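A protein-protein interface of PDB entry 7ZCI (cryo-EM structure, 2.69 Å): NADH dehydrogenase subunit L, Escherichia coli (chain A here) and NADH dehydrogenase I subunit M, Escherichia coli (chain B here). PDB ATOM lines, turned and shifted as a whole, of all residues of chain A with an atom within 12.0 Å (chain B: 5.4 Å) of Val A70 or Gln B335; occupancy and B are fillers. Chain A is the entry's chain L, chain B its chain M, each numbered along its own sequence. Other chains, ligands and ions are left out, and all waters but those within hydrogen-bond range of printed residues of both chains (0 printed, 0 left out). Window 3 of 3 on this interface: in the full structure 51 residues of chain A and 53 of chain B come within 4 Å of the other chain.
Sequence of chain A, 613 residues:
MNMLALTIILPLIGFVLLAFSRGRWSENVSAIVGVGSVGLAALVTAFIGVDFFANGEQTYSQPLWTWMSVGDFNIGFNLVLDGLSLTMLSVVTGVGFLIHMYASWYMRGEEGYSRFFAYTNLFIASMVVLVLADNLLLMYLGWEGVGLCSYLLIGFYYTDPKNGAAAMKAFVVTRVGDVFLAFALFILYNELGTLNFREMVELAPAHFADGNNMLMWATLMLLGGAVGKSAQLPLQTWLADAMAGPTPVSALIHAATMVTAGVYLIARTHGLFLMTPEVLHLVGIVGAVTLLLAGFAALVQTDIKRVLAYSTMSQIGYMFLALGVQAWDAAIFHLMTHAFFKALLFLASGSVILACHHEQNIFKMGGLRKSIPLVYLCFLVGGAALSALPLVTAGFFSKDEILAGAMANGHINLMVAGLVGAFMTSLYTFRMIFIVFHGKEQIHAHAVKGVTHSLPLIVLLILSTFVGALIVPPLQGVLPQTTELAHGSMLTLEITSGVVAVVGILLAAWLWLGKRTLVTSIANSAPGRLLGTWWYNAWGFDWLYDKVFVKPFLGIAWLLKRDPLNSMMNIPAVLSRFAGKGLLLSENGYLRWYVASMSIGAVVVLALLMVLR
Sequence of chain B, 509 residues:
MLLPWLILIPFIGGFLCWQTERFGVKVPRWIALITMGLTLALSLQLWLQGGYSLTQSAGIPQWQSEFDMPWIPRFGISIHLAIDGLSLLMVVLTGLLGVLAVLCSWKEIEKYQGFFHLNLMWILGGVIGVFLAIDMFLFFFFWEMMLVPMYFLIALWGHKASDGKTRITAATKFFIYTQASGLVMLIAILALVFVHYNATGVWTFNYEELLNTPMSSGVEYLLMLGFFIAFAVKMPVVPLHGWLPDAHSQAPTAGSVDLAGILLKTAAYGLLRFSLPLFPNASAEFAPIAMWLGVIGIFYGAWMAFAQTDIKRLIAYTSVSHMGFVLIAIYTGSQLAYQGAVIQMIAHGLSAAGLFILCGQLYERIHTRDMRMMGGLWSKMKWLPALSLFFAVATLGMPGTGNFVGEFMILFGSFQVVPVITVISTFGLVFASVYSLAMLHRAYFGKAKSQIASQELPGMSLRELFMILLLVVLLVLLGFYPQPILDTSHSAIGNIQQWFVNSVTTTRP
The side-chain amide nitrogen (NE2) of Gln B335 sits at hydrogen-bond distance from a ring nitrogen (ND1) of His B490, 3.0 Å away.
NE2 of Gln B339 sits at hydrogen-bond distance from O of Leu B486.
The side-chain hydroxyl (OH) of Tyr A189 sits close to the backbone NH (N) of Phe A73 (3.3 Å).
Val A70 touches Gln B335 (CG1 to NE2, 3.9 Å).
Leu B336 touches Val A70.
Val A70 touches Gln B339.
CG2 of Val A70 touches SD of Met B409, 3.9 Å away.
Phe A73 touches Leu B336.
CE2 of Phe A73 touches CG of Met B409, 3.8 Å away.
Met A68 touches none of the printed residues of chain B.
Val A70 touches just these residues of chain B: Gln B335 (3.9 Å), Leu B336 (3.7 Å), Gln B339 (3.8 Å) and Met B409 (3.9 Å).
Of the printed residues of chain B, Phe A73 touches Leu B336 (3.6 Å) and Met B409 (3.8 Å).
No residue of chain A comes within 4 Å of Gly B333.
Ser B334 touches none of the printed residues of chain A.
Leu B336 touches just these residues of chain A: Val A70 and Phe A73.
No residue of chain A comes within 4 Å of Ala B337.
No residue of chain A comes within 4 Å of Tyr B338.
Gln B339 touches one residue of chain A.
Of the printed residues of chain A, Met B409 touches Val A70 and Phe A73.
No residue of chain A comes within 4 Å of His B490.
No residue of chain A comes within 4 Å of Ile B493.
No residue of chain A comes within 4 Å of Gly B494.
The nearest residue of chain B that does not touch Val A70 is Leu B486 (4.04 Å).
Of the 19 printed residues of chain A, 2 touch a printed residue of chain B.
Hydrophobic or aromatic side chains of chain A that line the printed part of chain B: Val A70 and Phe A73.
Along chain A the printed residues that touch a printed residue of chain B span positions 70 to 73.
Printed residues of chain B that touch a printed residue of chain A: Gln B335, Leu B336, Gln B339 and Met B409.
Among the printed residues, 6 pairs touch across the chains.
Among the printed residues, no Asp or Glu carboxylate lies within 4 Å of a Lys or Arg side-chain nitrogen of the other chain.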
ATOM      1  N   THR A  66       2.096  -3.107  15.759  1.00  0.00           N
ATOM      2  CA  THR A  66       1.870  -3.404  14.350  1.00  0.00           C
ATOM      3  C   THR A  66       2.045  -2.119  13.557  1.00  0.00           C
ATOM      4  O   THR A  66       1.361  -1.126  13.822  1.00  0.00           O
ATOM      5  CB  THR A  66       0.479  -3.994  14.118  1.00  0.00           C
ATOM      6  OG1 THR A  66       0.394  -5.281  14.739  1.00  0.00           O
ATOM      7  CG2 THR A  66       0.205  -4.138  12.636  1.00  0.00           C
ATOM      8  N   TRP A  67       2.959  -2.141  12.590  1.00  0.00           N
ATOM      9  CA  TRP A  67       3.272  -0.928  11.848  1.00  0.00           C
ATOM     10  C   TRP A  67       2.152  -0.573  10.881  1.00  0.00           C
ATOM     11  O   TRP A  67       1.500   0.467  11.021  1.00  0.00           O
ATOM     12  CB  TRP A  67       4.595  -1.105  11.106  1.00  0.00           C
ATOM     13  CG  TRP A  67       5.237   0.171  10.710  1.00  0.00           C
ATOM     14  CD1 TRP A  67       4.832   1.426  11.034  1.00  0.00           C
ATOM     15  CD2 TRP A  67       6.400   0.322   9.896  1.00  0.00           C
ATOM     16  NE1 TRP A  67       5.671   2.353  10.476  1.00  0.00           N
ATOM     17  CE2 TRP A  67       6.644   1.698   9.771  1.00  0.00           C
ATOM     18  CE3 TRP A  67       7.263  -0.577   9.264  1.00  0.00           C
ATOM     19  CZ2 TRP A  67       7.715   2.200   9.042  1.00  0.00           C
ATOM     20  CZ3 TRP A  67       8.321  -0.077   8.542  1.00  0.00           C
ATOM     21  CH2 TRP A  67       8.539   1.296   8.436  1.00  0.00           C
ATOM     22  N   MET A  68       1.904  -1.428   9.895  1.00  0.00           N
ATOM     23  CA  MET A  68       0.881  -1.174   8.891  1.00  0.00           C
ATOM     24  C   MET A  68       0.005  -2.405   8.731  1.00  0.00           C
ATOM     25  O   MET A  68       0.469  -3.537   8.870  1.00  0.00           O
ATOM     26  CB  MET A  68       1.486  -0.792   7.526  1.00  0.00           C
ATOM     27  CG  MET A  68       2.643   0.188   7.593  1.00  0.00           C
ATOM     28  SD  MET A  68       3.652   0.218   6.109  1.00  0.00           S
ATOM     29  CE  MET A  68       4.936   1.353   6.619  1.00  0.00           C
ATOM     30  N   SER A  69      -1.270  -2.175   8.431  1.00  0.00           N
ATOM     31  CA  SER A  69      -2.207  -3.279   8.241  1.00  0.00           C
ATOM     32  C   SER A  69      -3.279  -2.825   7.254  1.00  0.00           C
ATOM     33  O   SER A  69      -4.245  -2.164   7.644  1.00  0.00           O
ATOM     34  CB  SER A  69      -2.813  -3.713   9.567  1.00  0.00           C
ATOM     35  OG  SER A  69      -3.689  -4.807   9.384  1.00  0.00           O
ATOM     36  N   VAL A  70      -3.098  -3.182   5.988  1.00  0.00           N
ATOM     37  CA  VAL A  70      -4.079  -2.941   4.935  1.00  0.00           C
ATOM     38  C   VAL A  70      -4.379  -4.297   4.313  1.00  0.00           C
ATOM     39  O   VAL A  70      -3.640  -4.766   3.439  1.00  0.00           O
ATOM     40  CB  VAL A  70      -3.582  -1.944   3.881  1.00  0.00           C
ATOM     41  CG1 VAL A  70      -4.650  -1.716   2.830  1.00  0.00           C
ATOM     42  CG2 VAL A  70      -3.197  -0.630   4.522  1.00  0.00           C
ATOM     43  N   GLY A  71      -5.455  -4.935   4.767  1.00  0.00           N
ATOM     44  CA  GLY A  71      -5.856  -6.226   4.244  1.00  0.00           C
ATOM     45  C   GLY A  71      -4.858  -7.332   4.516  1.00  0.00           C
ATOM     46  O   GLY A  71      -4.595  -7.675   5.671  1.00  0.00           O
ATOM     47  N   ASP A  72      -4.300  -7.902   3.449  1.00  0.00           N
ATOM     48  CA  ASP A  72      -3.251  -8.900   3.583  1.00  0.00           C
ATOM     49  C   ASP A  72      -1.880  -8.285   3.822  1.00  0.00           C
ATOM     50  O   ASP A  72      -0.952  -9.009   4.198  1.00  0.00           O
ATOM     51  CB  ASP A  72      -3.210  -9.782   2.337  1.00  0.00           C
ATOM     52  CG  ASP A  72      -4.503 -10.541   2.121  1.00  0.00           C
ATOM     53  OD1 ASP A  72      -5.131 -10.943   3.121  1.00  0.00           O
ATOM     54  OD2 ASP A  72      -4.893 -10.734   0.951  1.00  0.00           O
ATOM     55  N   PHE A  73      -1.735  -6.980   3.618  1.00  0.00           N
ATOM     56  CA  PHE A  73      -0.487  -6.261   3.858  1.00  0.00           C
ATOM     57  C   PHE A  73      -0.378  -5.996   5.350  1.00  0.00           C
ATOM     58  O   PHE A  73      -0.898  -5.010   5.863  1.00  0.00           O
ATOM     59  CB  PHE A  73      -0.469  -4.966   3.060  1.00  0.00           C
ATOM     60  CG  PHE A  73       0.821  -4.215   3.134  1.00  0.00           C
ATOM     61  CD1 PHE A  73       1.897  -4.588   2.356  1.00  0.00           C
ATOM     62  CD2 PHE A  73       0.948  -3.114   3.958  1.00  0.00           C
ATOM     63  CE1 PHE A  73       3.077  -3.891   2.413  1.00  0.00           C
ATOM     64  CE2 PHE A  73       2.127  -2.413   4.015  1.00  0.00           C
ATOM     65  CZ  PHE A  73       3.191  -2.801   3.240  1.00  0.00           C
ATOM     66  N   ASN A  74       0.298  -6.890   6.060  1.00  0.00           N
ATOM     67  CA  ASN A  74       0.413  -6.808   7.513  1.00  0.00           C
ATOM     68  C   ASN A  74       1.892  -6.736   7.867  1.00  0.00           C
ATOM     69  O   ASN A  74       2.565  -7.761   7.979  1.00  0.00           O
ATOM     70  CB  ASN A  74      -0.271  -7.992   8.178  1.00  0.00           C
ATOM     71  CG  ASN A  74      -0.435  -7.805   9.668  1.00  0.00           C
ATOM     72  OD1 ASN A  74      -0.273  -6.705  10.189  1.00  0.00           O
ATOM     73  ND2 ASN A  74      -0.763  -8.884  10.366  1.00  0.00           N
ATOM     74  N   ILE A  75       2.393  -5.520   8.048  1.00  0.00           N
ATOM     75  CA  ILE A  75       3.790  -5.279   8.381  1.00  0.00           C
ATOM     76  C   ILE A  75       3.874  -4.968   9.866  1.00  0.00           C
ATOM     77  O   ILE A  75       3.269  -3.999  10.343  1.00  0.00           O
ATOM     78  CB  ILE A  75       4.374  -4.134   7.542  1.00  0.00           C
ATOM     79  CG1 ILE A  75       4.476  -4.555   6.077  1.00  0.00           C
ATOM     80  CG2 ILE A  75       5.721  -3.708   8.089  1.00  0.00           C
ATOM     81  CD1 ILE A  75       5.251  -5.827   5.850  1.00  0.00           C
ATOM     82  N   GLY A  76       4.625  -5.788  10.592  1.00  0.00           N
ATOM     83  CA  GLY A  76       4.721  -5.682  12.032  1.00  0.00           C
ATOM     84  C   GLY A  76       5.979  -4.971  12.492  1.00  0.00           C
ATOM     85  O   GLY A  76       7.005  -4.981  11.820  1.00  0.00           O
ATOM     86  N   PHE A  77       5.875  -4.339  13.656  1.00  0.00           N
ATOM     87  CA  PHE A  77       7.007  -3.679  14.296  1.00  0.00           C
ATOM     88  C   PHE A  77       7.588  -4.614  15.356  1.00  0.00           C
ATOM     89  O   PHE A  77       7.494  -4.388  16.560  1.00  0.00           O
ATOM     90  CB  PHE A  77       6.556  -2.353  14.898  1.00  0.00           C
ATOM     91  CG  PHE A  77       7.555  -1.259  14.780  1.00  0.00           C
ATOM     92  CD1 PHE A  77       8.734  -1.298  15.499  1.00  0.00           C
ATOM     93  CD2 PHE A  77       7.310  -0.178  13.956  1.00  0.00           C
ATOM     94  CE1 PHE A  77       9.647  -0.279  15.392  1.00  0.00           C
ATOM     95  CE2 PHE A  77       8.217   0.842  13.847  1.00  0.00           C
ATOM     96  CZ  PHE A  77       9.385   0.791  14.564  1.00  0.00           C
ATOM     97  N   ASN A 135      11.229  -8.323   9.900  1.00  0.00           N
ATOM     98  CA  ASN A 135      10.674  -8.242   8.558  1.00  0.00           C
ATOM     99  C   ASN A 135      11.518  -7.296   7.720  1.00  0.00           C
ATOM    100  O   ASN A 135      12.320  -6.514   8.235  1.00  0.00           O
ATOM    101  CB  ASN A 135       9.212  -7.777   8.575  1.00  0.00           C
ATOM    102  CG  ASN A 135       8.984  -6.624   9.519  1.00  0.00           C
ATOM    103  OD1 ASN A 135       9.876  -6.241  10.267  1.00  0.00           O
ATOM    104  ND2 ASN A 135       7.790  -6.063   9.490  1.00  0.00           N
ATOM    105  N   LEU A 137      10.636  -4.713   5.858  1.00  0.00           N
ATOM    106  CA  LEU A 137      10.304  -3.290   5.848  1.00  0.00           C
ATOM    107  C   LEU A 137      10.884  -2.548   7.052  1.00  0.00           C
ATOM    108  O   LEU A 137      11.331  -1.404   6.922  1.00  0.00           O
ATOM    109  CB  LEU A 137       8.787  -3.111   5.777  1.00  0.00           C
ATOM    110  CG  LEU A 137       8.264  -1.750   5.311  1.00  0.00           C
ATOM    111  CD1 LEU A 137       9.048  -1.225   4.132  1.00  0.00           C
ATOM    112  CD2 LEU A 137       6.799  -1.842   4.956  1.00  0.00           C
ATOM    113  N   TYR A 189       6.874  -9.291  -1.715  1.00  0.00           N
ATOM    114  CA  TYR A 189       5.516  -9.186  -1.193  1.00  0.00           C
ATOM    115  C   TYR A 189       4.480  -9.553  -2.249  1.00  0.00           C
ATOM    116  O   TYR A 189       3.458 -10.168  -1.929  1.00  0.00           O
ATOM    117  CB  TYR A 189       5.239  -7.787  -0.652  1.00  0.00           C
ATOM    118  CG  TYR A 189       3.789  -7.612  -0.275  1.00  0.00           C
ATOM    119  CD1 TYR A 189       3.267  -8.245   0.844  1.00  0.00           C
ATOM    120  CD2 TYR A 189       2.929  -6.857  -1.063  1.00  0.00           C
ATOM    121  CE1 TYR A 189       1.939  -8.111   1.180  1.00  0.00           C
ATOM    122  CE2 TYR A 189       1.602  -6.722  -0.736  1.00  0.00           C
ATOM    123  CZ  TYR A 189       1.113  -7.350   0.384  1.00  0.00           C
ATOM    124  OH  TYR A 189      -0.212  -7.212   0.711  1.00  0.00           O
ATOM    125  N   ASN A 190       4.717  -9.184  -3.513  1.00  0.00           N
ATOM    126  CA  ASN A 190       3.781  -9.560  -4.565  1.00  0.00           C
ATOM    127  C   ASN A 190       3.741 -11.066  -4.774  1.00  0.00           C
ATOM    128  O   ASN A 190       2.687 -11.613  -5.113  1.00  0.00           O
ATOM    129  CB  ASN A 190       4.146  -8.869  -5.874  1.00  0.00           C
ATOM    130  CG  ASN A 190       3.114  -9.092  -6.954  1.00  0.00           C
ATOM    131  OD1 ASN A 190       1.919  -9.164  -6.679  1.00  0.00           O
ATOM    132  ND2 ASN A 190       3.572  -9.217  -8.192  1.00  0.00           N
ATOM    133  N   GLY A 193       3.296 -12.532  -0.304  1.00  0.00           N
ATOM    134  CA  GLY A 193       2.317 -11.947   0.584  1.00  0.00           C
ATOM    135  C   GLY A 193       2.802 -11.656   1.981  1.00  0.00           C
ATOM    136  O   GLY A 193       1.982 -11.345   2.850  1.00  0.00           O
ATOM    137  N   THR A 194       4.105 -11.753   2.231  1.00  0.00           N
ATOM    138  CA  THR A 194       4.663 -11.429   3.533  1.00  0.00           C
ATOM    139  C   THR A 194       6.084 -10.927   3.345  1.00  0.00           C
ATOM    140  O   THR A 194       6.716 -11.169   2.316  1.00  0.00           O
ATOM    141  CB  THR A 194       4.647 -12.637   4.478  1.00  0.00           C
ATOM    142  OG1 THR A 194       5.303 -12.294   5.702  1.00  0.00           O
ATOM    143  CG2 THR A 194       5.357 -13.816   3.846  1.00  0.00           C
ATOM    144  N   LEU A 195       6.574 -10.204   4.349  1.00  0.00           N
ATOM    145  CA  LEU A 195       7.952  -9.743   4.362  1.00  0.00           C
ATOM    146  C   LEU A 195       8.727 -10.240   5.573  1.00  0.00           C
ATOM    147  O   LEU A 195       9.890  -9.860   5.741  1.00  0.00           O
ATOM    148  CB  LEU A 195       8.013  -8.213   4.301  1.00  0.00           C
ATOM    149  CG  LEU A 195       7.601  -7.597   2.964  1.00  0.00           C
ATOM    150  CD1 LEU A 195       7.768  -6.096   2.989  1.00  0.00           C
ATOM    151  CD2 LEU A 195       8.383  -8.207   1.813  1.00  0.00           C
ATOM    152  N   GLY B 333      -5.986  -0.375  -9.237  1.00  0.00           N
ATOM    153  CA  GLY B 333      -7.179  -0.984  -8.688  1.00  0.00           C
ATOM    154  C   GLY B 333      -6.938  -1.543  -7.305  1.00  0.00           C
ATOM    155  O   GLY B 333      -7.676  -2.417  -6.842  1.00  0.00           O
ATOM    156  N   SER B 334      -5.908  -1.037  -6.632  1.00  0.00           N
ATOM    157  CA  SER B 334      -5.420  -1.610  -5.387  1.00  0.00           C
ATOM    158  C   SER B 334      -5.952  -0.831  -4.194  1.00  0.00           C
ATOM    159  O   SER B 334      -5.917   0.401  -4.183  1.00  0.00           O
ATOM    160  CB  SER B 334      -3.893  -1.619  -5.357  1.00  0.00           C
ATOM    161  OG  SER B 334      -3.374  -2.679  -6.137  1.00  0.00           O
ATOM    162  N   GLN B 335      -6.447  -1.561  -3.196  1.00  0.00           N
ATOM    163  CA  GLN B 335      -6.809  -0.938  -1.931  1.00  0.00           C
ATOM    164  C   GLN B 335      -5.573  -0.445  -1.190  1.00  0.00           C
ATOM    165  O   GLN B 335      -5.609   0.603  -0.533  1.00  0.00           O
ATOM    166  CB  GLN B 335      -7.594  -1.932  -1.080  1.00  0.00           C
ATOM    167  CG  GLN B 335      -8.381  -1.300   0.040  1.00  0.00           C
ATOM    168  CD  GLN B 335      -8.305  -2.094   1.321  1.00  0.00           C
ATOM    169  OE1 GLN B 335      -8.078  -3.304   1.304  1.00  0.00           O
ATOM    170  NE2 GLN B 335      -8.489  -1.416   2.446  1.00  0.00           N
ATOM    171  N   LEU B 336      -4.472  -1.195  -1.285  1.00  0.00           N
ATOM    172  CA  LEU B 336      -3.227  -0.813  -0.628  1.00  0.00           C
ATOM    173  C   LEU B 336      -2.663   0.477  -1.207  1.00  0.00           C
ATOM    174  O   LEU B 336      -2.215   1.354  -0.461  1.00  0.00           O
ATOM    175  CB  LEU B 336      -2.213  -1.948  -0.756  1.00  0.00           C
ATOM    176  CG  LEU B 336      -0.819  -1.745  -0.174  1.00  0.00           C
ATOM    177  CD1 LEU B 336      -0.915  -1.490   1.302  1.00  0.00           C
ATOM    178  CD2 LEU B 336       0.029  -2.963  -0.446  1.00  0.00           C
ATOM    179  N   ALA B 337      -2.696   0.617  -2.532  1.00  0.00           N
ATOM    180  CA  ALA B 337      -2.234   1.848  -3.157  1.00  0.00           C
ATOM    181  C   ALA B 337      -3.135   3.030  -2.819  1.00  0.00           C
ATOM    182  O   ALA B 337      -2.643   4.152  -2.681  1.00  0.00           O
ATOM    183  CB  ALA B 337      -2.137   1.668  -4.667  1.00  0.00           C
ATOM    184  N   TYR B 338      -4.443   2.807  -2.657  1.00  0.00           N
ATOM    185  CA  TYR B 338      -5.329   3.910  -2.288  1.00  0.00           C
ATOM    186  C   TYR B 338      -5.088   4.350  -0.850  1.00  0.00           C
ATOM    187  O   TYR B 338      -5.112   5.551  -0.549  1.00  0.00           O
ATOM    188  CB  TYR B 338      -6.798   3.522  -2.463  1.00  0.00           C
ATOM    189  CG  TYR B 338      -7.271   3.263  -3.873  1.00  0.00           C
ATOM    190  CD1 TYR B 338      -6.456   3.503  -4.965  1.00  0.00           C
ATOM    191  CD2 TYR B 338      -8.549   2.774  -4.108  1.00  0.00           C
ATOM    192  CE1 TYR B 338      -6.889   3.250  -6.240  1.00  0.00           C
ATOM    193  CE2 TYR B 338      -8.992   2.525  -5.384  1.00  0.00           C
ATOM    194  CZ  TYR B 338      -8.157   2.767  -6.446  1.00  0.00           C
ATOM    195  OH  TYR B 338      -8.582   2.522  -7.727  1.00  0.00           O
ATOM    196  N   GLN B 339      -4.870   3.393   0.054  1.00  0.00           N
ATOM    197  CA  GLN B 339      -4.536   3.743   1.430  1.00  0.00           C
ATOM    198  C   GLN B 339      -3.204   4.478   1.498  1.00  0.00           C
ATOM    199  O   GLN B 339      -3.049   5.438   2.268  1.00  0.00           O
ATOM    200  CB  GLN B 339      -4.506   2.487   2.294  1.00  0.00           C
ATOM    201  CG  GLN B 339      -5.868   1.890   2.564  1.00  0.00           C
ATOM    202  CD  GLN B 339      -6.563   2.544   3.732  1.00  0.00           C
ATOM    203  OE1 GLN B 339      -7.015   3.682   3.641  1.00  0.00           O
ATOM    204  NE2 GLN B 339      -6.640   1.833   4.845  1.00  0.00           N
ATOM    205  N   GLY B 340      -2.238   4.053   0.683  1.00  0.00           N
ATOM    206  CA  GLY B 340      -0.992   4.790   0.581  1.00  0.00           C
ATOM    207  C   GLY B 340      -1.183   6.186   0.029  1.00  0.00           C
ATOM    208  O   GLY B 340      -0.504   7.121   0.445  1.00  0.00           O
ATOM    209  N   MET B 409       3.525   2.367   0.459  1.00  0.00           N
ATOM    210  CA  MET B 409       2.292   1.614   0.258  1.00  0.00           C
ATOM    211  C   MET B 409       1.735   1.847  -1.142  1.00  0.00           C
ATOM    212  O   MET B 409       1.209   0.911  -1.769  1.00  0.00           O
ATOM    213  CB  MET B 409       1.278   1.972   1.341  1.00  0.00           C
ATOM    214  CG  MET B 409       1.386   1.060   2.551  1.00  0.00           C
ATOM    215  SD  MET B 409       0.136   1.258   3.836  1.00  0.00           S
ATOM    216  CE  MET B 409      -0.311   2.966   3.635  1.00  0.00           C
ATOM    217  N   LEU B 486      -5.297   4.705   8.689  1.00  0.00           N
ATOM    218  CA  LEU B 486      -5.727   3.627   7.809  1.00  0.00           C
ATOM    219  C   LEU B 486      -7.075   3.068   8.241  1.00  0.00           C
ATOM    220  O   LEU B 486      -7.935   2.785   7.400  1.00  0.00           O
ATOM    221  CB  LEU B 486      -4.674   2.523   7.784  1.00  0.00           C
ATOM    222  CG  LEU B 486      -3.282   2.935   7.312  1.00  0.00           C
ATOM    223  CD1 LEU B 486      -2.288   1.832   7.593  1.00  0.00           C
ATOM    224  CD2 LEU B 486      -3.302   3.274   5.842  1.00  0.00           C
ATOM    225  N   HIS B 490     -10.354   3.246   5.851  1.00  0.00           N
ATOM    226  CA  HIS B 490     -10.454   1.895   5.305  1.00  0.00           C
ATOM    227  C   HIS B 490     -11.790   1.636   4.618  1.00  0.00           C
ATOM    228  O   HIS B 490     -11.825   1.109   3.502  1.00  0.00           O
ATOM    229  CB  HIS B 490     -10.226   0.878   6.420  1.00  0.00           C
ATOM    230  CG  HIS B 490     -10.446  -0.538   5.997  1.00  0.00           C
ATOM    231  ND1 HIS B 490      -9.493  -1.268   5.321  1.00  0.00           N
ATOM    232  CD2 HIS B 490     -11.508  -1.361   6.156  1.00  0.00           C
ATOM    233  CE1 HIS B 490      -9.960  -2.479   5.079  1.00  0.00           C
ATOM    234  NE2 HIS B 490     -11.181  -2.562   5.574  1.00  0.00           N
ATOM    235  N   ILE B 493     -12.258   3.811   1.386  1.00  0.00           N
ATOM    236  CA  ILE B 493     -11.366   3.348   0.331  1.00  0.00           C
ATOM    237  C   ILE B 493     -11.837   2.007  -0.214  1.00  0.00           C
ATOM    238  O   ILE B 493     -11.791   1.763  -1.426  1.00  0.00           O
ATOM    239  CB  ILE B 493      -9.924   3.299   0.871  1.00  0.00           C
ATOM    240  CG1 ILE B 493      -9.330   4.708   0.894  1.00  0.00           C
ATOM    241  CG2 ILE B 493      -9.057   2.341   0.089  1.00  0.00           C
ATOM    242  CD1 ILE B 493      -9.361   5.410  -0.436  1.00  0.00           C
ATOM    243  N   GLY B 494     -12.328   1.132   0.664  1.00  0.00           N
ATOM    244  CA  GLY B 494     -12.858  -0.143   0.214  1.00  0.00           C
ATOM    245  C   GLY B 494     -14.098   0.005  -0.643  1.00  0.00           C
ATOM    246  O   GLY B 494     -14.260  -0.709  -1.634  1.00  0.00           O
ATOM    247  N   GLN B 497     -12.850   1.381  -4.098  1.00  0.00           N
ATOM    248  CA  GLN B 497     -12.128   0.358  -4.844  1.00  0.00           C
ATOM    249  C   GLN B 497     -13.053  -0.755  -5.316  1.00  0.00           C
ATOM    250  O   GLN B 497     -12.934  -1.220  -6.455  1.00  0.00           O
ATOM    251  CB  GLN B 497     -10.998  -0.211  -3.987  1.00  0.00           C
ATOM    252  CG  GLN B 497     -10.079  -1.160  -4.726  1.00  0.00           C
ATOM    253  CD  GLN B 497     -10.412  -2.609  -4.471  1.00  0.00           C
ATOM    254  OE1 GLN B 497     -11.037  -2.947  -3.469  1.00  0.00           O
ATOM    255  NE2 GLN B 497      -9.999  -3.476  -5.382  1.00  0.00           N
